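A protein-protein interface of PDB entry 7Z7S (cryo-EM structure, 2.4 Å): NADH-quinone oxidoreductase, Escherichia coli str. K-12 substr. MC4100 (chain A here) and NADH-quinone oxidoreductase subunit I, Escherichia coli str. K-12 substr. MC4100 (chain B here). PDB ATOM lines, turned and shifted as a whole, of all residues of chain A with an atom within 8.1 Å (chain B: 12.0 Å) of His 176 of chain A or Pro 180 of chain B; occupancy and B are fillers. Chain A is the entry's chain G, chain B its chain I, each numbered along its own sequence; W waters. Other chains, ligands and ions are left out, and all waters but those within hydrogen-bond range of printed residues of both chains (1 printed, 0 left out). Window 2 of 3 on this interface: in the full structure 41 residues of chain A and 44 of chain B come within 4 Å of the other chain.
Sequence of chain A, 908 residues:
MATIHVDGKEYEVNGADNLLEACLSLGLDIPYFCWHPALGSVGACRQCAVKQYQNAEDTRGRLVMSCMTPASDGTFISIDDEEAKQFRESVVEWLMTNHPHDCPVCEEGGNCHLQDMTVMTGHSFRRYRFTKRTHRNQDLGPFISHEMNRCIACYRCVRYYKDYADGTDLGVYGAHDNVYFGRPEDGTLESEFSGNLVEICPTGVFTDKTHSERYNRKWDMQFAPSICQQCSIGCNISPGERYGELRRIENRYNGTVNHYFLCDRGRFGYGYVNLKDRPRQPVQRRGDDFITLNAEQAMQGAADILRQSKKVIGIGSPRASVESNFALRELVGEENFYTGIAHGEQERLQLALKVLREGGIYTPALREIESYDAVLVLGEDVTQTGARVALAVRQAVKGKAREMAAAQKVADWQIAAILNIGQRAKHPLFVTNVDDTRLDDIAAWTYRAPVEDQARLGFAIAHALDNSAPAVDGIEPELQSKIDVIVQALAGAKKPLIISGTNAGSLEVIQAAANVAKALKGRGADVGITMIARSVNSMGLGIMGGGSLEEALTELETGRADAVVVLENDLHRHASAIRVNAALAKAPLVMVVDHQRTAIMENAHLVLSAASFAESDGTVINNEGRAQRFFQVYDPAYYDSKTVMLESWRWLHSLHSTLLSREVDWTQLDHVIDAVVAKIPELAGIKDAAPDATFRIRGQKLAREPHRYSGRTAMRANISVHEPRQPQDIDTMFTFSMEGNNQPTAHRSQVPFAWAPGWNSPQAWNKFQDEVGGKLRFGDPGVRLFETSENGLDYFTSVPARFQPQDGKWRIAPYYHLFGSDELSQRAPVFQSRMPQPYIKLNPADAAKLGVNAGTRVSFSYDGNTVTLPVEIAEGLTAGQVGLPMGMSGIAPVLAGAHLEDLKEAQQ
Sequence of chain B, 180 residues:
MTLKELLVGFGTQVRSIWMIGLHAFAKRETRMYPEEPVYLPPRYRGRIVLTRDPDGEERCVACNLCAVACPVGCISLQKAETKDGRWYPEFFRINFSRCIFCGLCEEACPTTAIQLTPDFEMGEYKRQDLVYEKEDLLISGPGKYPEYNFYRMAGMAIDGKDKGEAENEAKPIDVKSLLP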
ATOM      1  N   ALA A 153      -6.206 -33.133 -25.467  1.00  0.00           N
ATOM      2  CA  ALA A 153      -5.152 -34.084 -25.098  1.00  0.00           C
ATOM      3  C   ALA A 153      -5.642 -35.526 -25.196  1.00  0.00           C
ATOM      4  O   ALA A 153      -5.531 -36.313 -24.261  1.00  0.00           O
ATOM      5  CB  ALA A 153      -4.584 -33.784 -23.710  1.00  0.00           C
ATOM      6  N   TYR A 155      -4.515 -37.562 -27.607  1.00  0.00           N
ATOM      7  CA  TYR A 155      -3.350 -38.261 -28.145  1.00  0.00           C
ATOM      8  C   TYR A 155      -3.610 -38.935 -29.486  1.00  0.00           C
ATOM      9  O   TYR A 155      -2.783 -39.721 -29.930  1.00  0.00           O
ATOM     10  CB  TYR A 155      -2.786 -39.292 -27.153  1.00  0.00           C
ATOM     11  CG  TYR A 155      -2.220 -38.678 -25.901  1.00  0.00           C
ATOM     12  CD1 TYR A 155      -3.042 -38.324 -24.845  1.00  0.00           C
ATOM     13  CD2 TYR A 155      -0.861 -38.442 -25.780  1.00  0.00           C
ATOM     14  CE1 TYR A 155      -2.529 -37.751 -23.709  1.00  0.00           C
ATOM     15  CE2 TYR A 155      -0.341 -37.876 -24.651  1.00  0.00           C
ATOM     16  CZ  TYR A 155      -1.175 -37.533 -23.618  1.00  0.00           C
ATOM     17  OH  TYR A 155      -0.657 -36.966 -22.487  1.00  0.00           O
ATOM     18  N   TYR A 173       4.717 -32.871 -26.052  1.00  0.00           N
ATOM     19  CA  TYR A 173       5.711 -32.217 -25.222  1.00  0.00           C
ATOM     20  C   TYR A 173       5.053 -31.700 -23.959  1.00  0.00           C
ATOM     21  O   TYR A 173       3.831 -31.600 -23.859  1.00  0.00           O
ATOM     22  CB  TYR A 173       6.397 -31.076 -25.978  1.00  0.00           C
ATOM     23  CG  TYR A 173       6.658 -31.443 -27.402  1.00  0.00           C
ATOM     24  CD1 TYR A 173       7.665 -32.337 -27.727  1.00  0.00           C
ATOM     25  CD2 TYR A 173       5.869 -30.942 -28.420  1.00  0.00           C
ATOM     26  CE1 TYR A 173       7.893 -32.702 -29.024  1.00  0.00           C
ATOM     27  CE2 TYR A 173       6.089 -31.303 -29.719  1.00  0.00           C
ATOM     28  CZ  TYR A 173       7.101 -32.180 -30.015  1.00  0.00           C
ATOM     29  OH  TYR A 173       7.316 -32.539 -31.314  1.00  0.00           O
ATOM     30  N   GLY A 174       5.883 -31.380 -22.988  1.00  0.00           N
ATOM     31  CA  GLY A 174       5.390 -30.874 -21.740  1.00  0.00           C
ATOM     32  C   GLY A 174       4.832 -31.974 -20.861  1.00  0.00           C
ATOM     33  O   GLY A 174       5.110 -33.157 -21.021  1.00  0.00           O
ATOM     34  N   ALA A 175       3.989 -31.551 -19.934  1.00  0.00           N
ATOM     35  CA  ALA A 175       3.539 -32.377 -18.832  1.00  0.00           C
ATOM     36  C   ALA A 175       2.124 -31.942 -18.487  1.00  0.00           C
ATOM     37  O   ALA A 175       1.437 -31.326 -19.307  1.00  0.00           O
ATOM     38  CB  ALA A 175       4.513 -32.294 -17.646  1.00  0.00           C
ATOM     39  N   HIS A 176       1.747 -32.153 -17.239  1.00  0.00           N
ATOM     40  CA  HIS A 176       0.425 -32.429 -16.697  1.00  0.00           C
ATOM     41  C   HIS A 176      -0.775 -31.842 -17.426  1.00  0.00           C
ATOM     42  O   HIS A 176      -1.370 -32.528 -18.250  1.00  0.00           O
ATOM     43  CB  HIS A 176       0.467 -31.831 -15.294  1.00  0.00           C
ATOM     44  CG  HIS A 176       1.391 -30.649 -15.205  1.00  0.00           C
ATOM     45  ND1 HIS A 176       0.997 -29.372 -15.538  1.00  0.00           N
ATOM     46  CD2 HIS A 176       2.707 -30.561 -14.892  1.00  0.00           C
ATOM     47  CE1 HIS A 176       2.018 -28.547 -15.409  1.00  0.00           C
ATOM     48  NE2 HIS A 176       3.068 -29.244 -15.019  1.00  0.00           N
ATOM     49  N   ASP A 177      -1.045 -30.557 -17.275  1.00  0.00           N
ATOM     50  CA  ASP A 177      -2.132 -29.927 -18.003  1.00  0.00           C
ATOM     51  C   ASP A 177      -1.596 -29.011 -19.080  1.00  0.00           C
ATOM     52  O   ASP A 177      -2.374 -28.357 -19.775  1.00  0.00           O
ATOM     53  CB  ASP A 177      -3.054 -29.154 -17.054  1.00  0.00           C
ATOM     54  CG  ASP A 177      -2.295 -28.214 -16.144  1.00  0.00           C
ATOM     55  OD1 ASP A 177      -2.015 -27.074 -16.568  1.00  0.00           O
ATOM     56  OD2 ASP A 177      -1.967 -28.616 -15.008  1.00  0.00           O
ATOM     57  N   ASN A 178      -0.279 -28.966 -19.232  1.00  0.00           N
ATOM     58  CA  ASN A 178       0.399 -28.178 -20.243  1.00  0.00           C
ATOM     59  C   ASN A 178       0.939 -29.047 -21.373  1.00  0.00           C
ATOM     60  O   ASN A 178       1.939 -28.695 -21.997  1.00  0.00           O
ATOM     61  CB  ASN A 178       1.528 -27.376 -19.602  1.00  0.00           C
ATOM     62  CG  ASN A 178       1.723 -26.033 -20.246  1.00  0.00           C
ATOM     63  OD1 ASN A 178       0.764 -25.368 -20.622  1.00  0.00           O
ATOM     64  ND2 ASN A 178       2.970 -25.626 -20.386  1.00  0.00           N
ATOM     65  N   VAL A 179       0.305 -30.192 -21.634  1.00  0.00           N
ATOM     66  CA  VAL A 179       0.742 -31.049 -22.730  1.00  0.00           C
ATOM     67  C   VAL A 179       0.463 -30.357 -24.056  1.00  0.00           C
ATOM     68  O   VAL A 179      -0.614 -29.792 -24.275  1.00  0.00           O
ATOM     69  CB  VAL A 179       0.070 -32.430 -22.665  1.00  0.00           C
ATOM     70  CG1 VAL A 179       0.848 -33.357 -21.750  1.00  0.00           C
ATOM     71  CG2 VAL A 179      -1.375 -32.322 -22.228  1.00  0.00           C
ATOM     72  N   TYR A 180       1.448 -30.389 -24.937  1.00  0.00           N
ATOM     73  CA  TYR A 180       1.432 -29.707 -26.216  1.00  0.00           C
ATOM     74  C   TYR A 180       1.610 -30.737 -27.316  1.00  0.00           C
ATOM     75  O   TYR A 180       2.442 -31.633 -27.204  1.00  0.00           O
ATOM     76  CB  TYR A 180       2.550 -28.676 -26.265  1.00  0.00           C
ATOM     77  CG  TYR A 180       2.422 -27.624 -27.327  1.00  0.00           C
ATOM     78  CD1 TYR A 180       2.936 -27.831 -28.598  1.00  0.00           C
ATOM     79  CD2 TYR A 180       1.816 -26.411 -27.055  1.00  0.00           C
ATOM     80  CE1 TYR A 180       2.838 -26.869 -29.568  1.00  0.00           C
ATOM     81  CE2 TYR A 180       1.711 -25.439 -28.021  1.00  0.00           C
ATOM     82  CZ  TYR A 180       2.224 -25.676 -29.276  1.00  0.00           C
ATOM     83  OH  TYR A 180       2.123 -24.713 -30.244  1.00  0.00           O
ATOM     84  N   ALA B 170      -5.626 -17.520 -18.770  1.00  0.00           N
ATOM     85  CA  ALA B 170      -4.291 -17.407 -18.213  1.00  0.00           C
ATOM     86  C   ALA B 170      -3.285 -17.194 -19.334  1.00  0.00           C
ATOM     87  O   ALA B 170      -3.546 -17.501 -20.497  1.00  0.00           O
ATOM     88  CB  ALA B 170      -3.930 -18.653 -17.409  1.00  0.00           C
ATOM     89  N   LYS B 171      -2.132 -16.646 -18.972  1.00  0.00           N
ATOM     90  CA  LYS B 171      -1.058 -16.480 -19.939  1.00  0.00           C
ATOM     91  C   LYS B 171      -0.538 -17.846 -20.378  1.00  0.00           C
ATOM     92  O   LYS B 171      -0.539 -18.791 -19.586  1.00  0.00           O
ATOM     93  CB  LYS B 171       0.080 -15.656 -19.348  1.00  0.00           C
ATOM     94  CG  LYS B 171       0.162 -14.252 -19.902  1.00  0.00           C
ATOM     95  CD  LYS B 171      -0.578 -13.264 -19.025  1.00  0.00           C
ATOM     96  CE  LYS B 171       0.273 -12.824 -17.851  1.00  0.00           C
ATOM     97  NZ  LYS B 171      -0.534 -12.105 -16.826  1.00  0.00           N
ATOM     98  N   PRO B 172      -0.126 -17.990 -21.635  1.00  0.00           N
ATOM     99  CA  PRO B 172       0.412 -19.277 -22.084  1.00  0.00           C
ATOM    100  C   PRO B 172       1.725 -19.607 -21.398  1.00  0.00           C
ATOM    101  O   PRO B 172       2.573 -18.741 -21.182  1.00  0.00           O
ATOM    102  CB  PRO B 172       0.598 -19.080 -23.592  1.00  0.00           C
ATOM    103  CG  PRO B 172       0.656 -17.621 -23.781  1.00  0.00           C
ATOM    104  CD  PRO B 172      -0.214 -17.019 -22.735  1.00  0.00           C
ATOM    105  N   ILE B 173       1.874 -20.877 -21.042  1.00  0.00           N
ATOM    106  CA  ILE B 173       3.076 -21.391 -20.406  1.00  0.00           C
ATOM    107  C   ILE B 173       3.788 -22.258 -21.426  1.00  0.00           C
ATOM    108  O   ILE B 173       3.204 -23.211 -21.952  1.00  0.00           O
ATOM    109  CB  ILE B 173       2.751 -22.191 -19.136  1.00  0.00           C
ATOM    110  CG1 ILE B 173       1.976 -21.331 -18.141  1.00  0.00           C
ATOM    111  CG2 ILE B 173       4.019 -22.739 -18.514  1.00  0.00           C
ATOM    112  CD1 ILE B 173       1.435 -22.109 -16.974  1.00  0.00           C
ATOM    113  N   ASP B 174       5.039 -21.922 -21.716  1.00  0.00           N
ATOM    114  CA  ASP B 174       5.832 -22.739 -22.616  1.00  0.00           C
ATOM    115  C   ASP B 174       6.143 -24.079 -21.966  1.00  0.00           C
ATOM    116  O   ASP B 174       6.288 -24.182 -20.747  1.00  0.00           O
ATOM    117  CB  ASP B 174       7.127 -22.022 -22.988  1.00  0.00           C
ATOM    118  CG  ASP B 174       7.686 -22.485 -24.316  1.00  0.00           C
ATOM    119  OD1 ASP B 174       8.407 -23.497 -24.335  1.00  0.00           O
ATOM    120  OD2 ASP B 174       7.404 -21.837 -25.343  1.00  0.00           O
ATOM    121  N   VAL B 175       6.233 -25.124 -22.794  1.00  0.00           N
ATOM    122  CA  VAL B 175       6.576 -26.441 -22.268  1.00  0.00           C
ATOM    123  C   VAL B 175       8.031 -26.509 -21.827  1.00  0.00           C
ATOM    124  O   VAL B 175       8.408 -27.422 -21.090  1.00  0.00           O
ATOM    125  CB  VAL B 175       6.277 -27.549 -23.296  1.00  0.00           C
ATOM    126  CG1 VAL B 175       4.791 -27.648 -23.543  1.00  0.00           C
ATOM    127  CG2 VAL B 175       7.033 -27.304 -24.593  1.00  0.00           C
ATOM    128  N   LYS B 176       8.853 -25.555 -22.245  1.00  0.00           N
ATOM    129  CA  LYS B 176      10.246 -25.473 -21.840  1.00  0.00           C
ATOM    130  C   LYS B 176      10.445 -24.697 -20.547  1.00  0.00           C
ATOM    131  O   LYS B 176      11.591 -24.475 -20.152  1.00  0.00           O
ATOM    132  CB  LYS B 176      11.073 -24.834 -22.952  1.00  0.00           C
ATOM    133  CG  LYS B 176      10.954 -25.542 -24.282  1.00  0.00           C
ATOM    134  CD  LYS B 176      12.150 -25.272 -25.163  1.00  0.00           C
ATOM    135  CE  LYS B 176      11.826 -24.294 -26.271  1.00  0.00           C
ATOM    136  NZ  LYS B 176      11.383 -22.981 -25.740  1.00  0.00           N
ATOM    137  N   SER B 177       9.368 -24.281 -19.889  1.00  0.00           N
ATOM    138  CA  SER B 177       9.472 -23.502 -18.665  1.00  0.00           C
ATOM    139  C   SER B 177      10.074 -24.328 -17.534  1.00  0.00           C
ATOM    140  O   SER B 177       9.852 -25.534 -17.428  1.00  0.00           O
ATOM    141  CB  SER B 177       8.099 -22.980 -18.248  1.00  0.00           C
ATOM    142  OG  SER B 177       7.406 -23.939 -17.476  1.00  0.00           O
ATOM    143  N   LEU B 178      10.850 -23.654 -16.685  1.00  0.00           N
ATOM    144  CA  LEU B 178      11.578 -24.335 -15.623  1.00  0.00           C
ATOM    145  C   LEU B 178      10.685 -24.755 -14.469  1.00  0.00           C
ATOM    146  O   LEU B 178      11.052 -25.668 -13.726  1.00  0.00           O
ATOM    147  CB  LEU B 178      12.701 -23.445 -15.101  1.00  0.00           C
ATOM    148  CG  LEU B 178      13.665 -22.893 -16.145  1.00  0.00           C
ATOM    149  CD1 LEU B 178      14.522 -21.801 -15.541  1.00  0.00           C
ATOM    150  CD2 LEU B 178      14.523 -24.005 -16.709  1.00  0.00           C
ATOM    151  N   LEU B 179       9.540 -24.110 -14.294  1.00  0.00           N
ATOM    152  CA  LEU B 179       8.655 -24.461 -13.195  1.00  0.00           C
ATOM    153  C   LEU B 179       8.008 -25.819 -13.459  1.00  0.00           C
ATOM    154  O   LEU B 179       7.612 -26.107 -14.590  1.00  0.00           O
ATOM    155  CB  LEU B 179       7.582 -23.392 -13.013  1.00  0.00           C
ATOM    156  CG  LEU B 179       8.092 -22.071 -12.441  1.00  0.00           C
ATOM    157  CD1 LEU B 179       7.051 -20.981 -12.579  1.00  0.00           C
ATOM    158  CD2 LEU B 179       8.489 -22.247 -10.994  1.00  0.00           C
ATOM    159  N   PRO B 180       7.893 -26.678 -12.434  1.00  0.00           N
ATOM    160  CA  PRO B 180       7.309 -28.018 -12.568  1.00  0.00           C
ATOM    161  C   PRO B 180       5.818 -27.999 -12.907  1.00  0.00           C
ATOM    162  O   PRO B 180       5.138 -27.001 -12.654  1.00  0.00           O
ATOM    163  CB  PRO B 180       7.536 -28.642 -11.186  1.00  0.00           C
ATOM    164  CG  PRO B 180       8.559 -27.789 -10.525  1.00  0.00           C
ATOM    165  CD  PRO B 180       8.353 -26.421 -11.061  1.00  0.00           C
HETATM  166  O   HOH W   1      -0.226 -23.034 -21.252  1.00  0.00           O
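The side-chain amide nitrogen (ND2) of Asn 178 of chain A sits at hydrogen-bond distance from the backbone carbonyl oxygen (O) of Ile 173 of chain B, 2.9 Å away.
The backbone NH (N) of Tyr 173 of chain A sits at hydrogen-bond distance from the backbone carbonyl oxygen (O) of Tyr 180 of chain A. OD1 of Asp 174 of chain B lies within salt-bridge range of NZ of Lys 176 of chain B. ND1 of His 176 of chain A lies within hydrogen-bond range of OD2 of Asp 177 of chain A, 3.1 Å away. O of Asp 174 of chain B lies close to OG of Ser 177 of chain B (3.5 Å).
Among the printed residues, merely in contact across the chains: Asn 178 of chain A with Val 175 of chain B, Asn 178 of chain A with Asp 174 of chain B, Tyr 180 of chain A with Val 175 of chain B, His 176 of chain A with Pro 180 of chain B and Gly 174 of chain A with Val 175 of chain B.
His 176 of chain A touches one residue of chain B. Pro 180 of chain B touches one residue of chain A. Of chain B, only Val 175 comes within 4 Å of Gly 174 of chain A. No residue of chain B comes within 4 Å of Ala 175 of chain A. No residue of chain B comes within 4 Å of Asp 177 of chain A. Of chain B, only Ile 173, Asp 174 and Val 175 come within 4 Å of Asn 178 of chain A. No residue of chain B comes within 4 Å of Val 179 of chain A. Printed residues of chain B within 4 Å of Tyr 180 of chain A: Val 175 (3.7 Å). Printed residues of chain A within 4 Å of Ile 173 of chain B: Asn 178 (2.9 Å). The nearest residue of chain A that does not touch Pro 180 of chain B is Ala 175 of chain A (6.5 Å).
Hydrophobic or aromatic side chains of chain A within 4 Å of the printed part of chain B: His 176 and Tyr 180. Printed residues of chain B that touch a printed residue of chain A: Ile 173, Asp 174, Val 175 and Pro 180. Hydrophobic or aromatic side chains of chain B within 4 Å of the printed part of chain A: Ile 173 and Val 175. Among the printed residues, 6 pairs touch across the chains. Among the printed residues, no Asp or Glu carboxylate lies within 4 Å of a Lys or Arg side-chain nitrogen of the other chain.
Water W1 bridges OD1 of Asn 178 of chain A (2.6 Å) and N of Ile 173 of chain B (3.0 Å).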
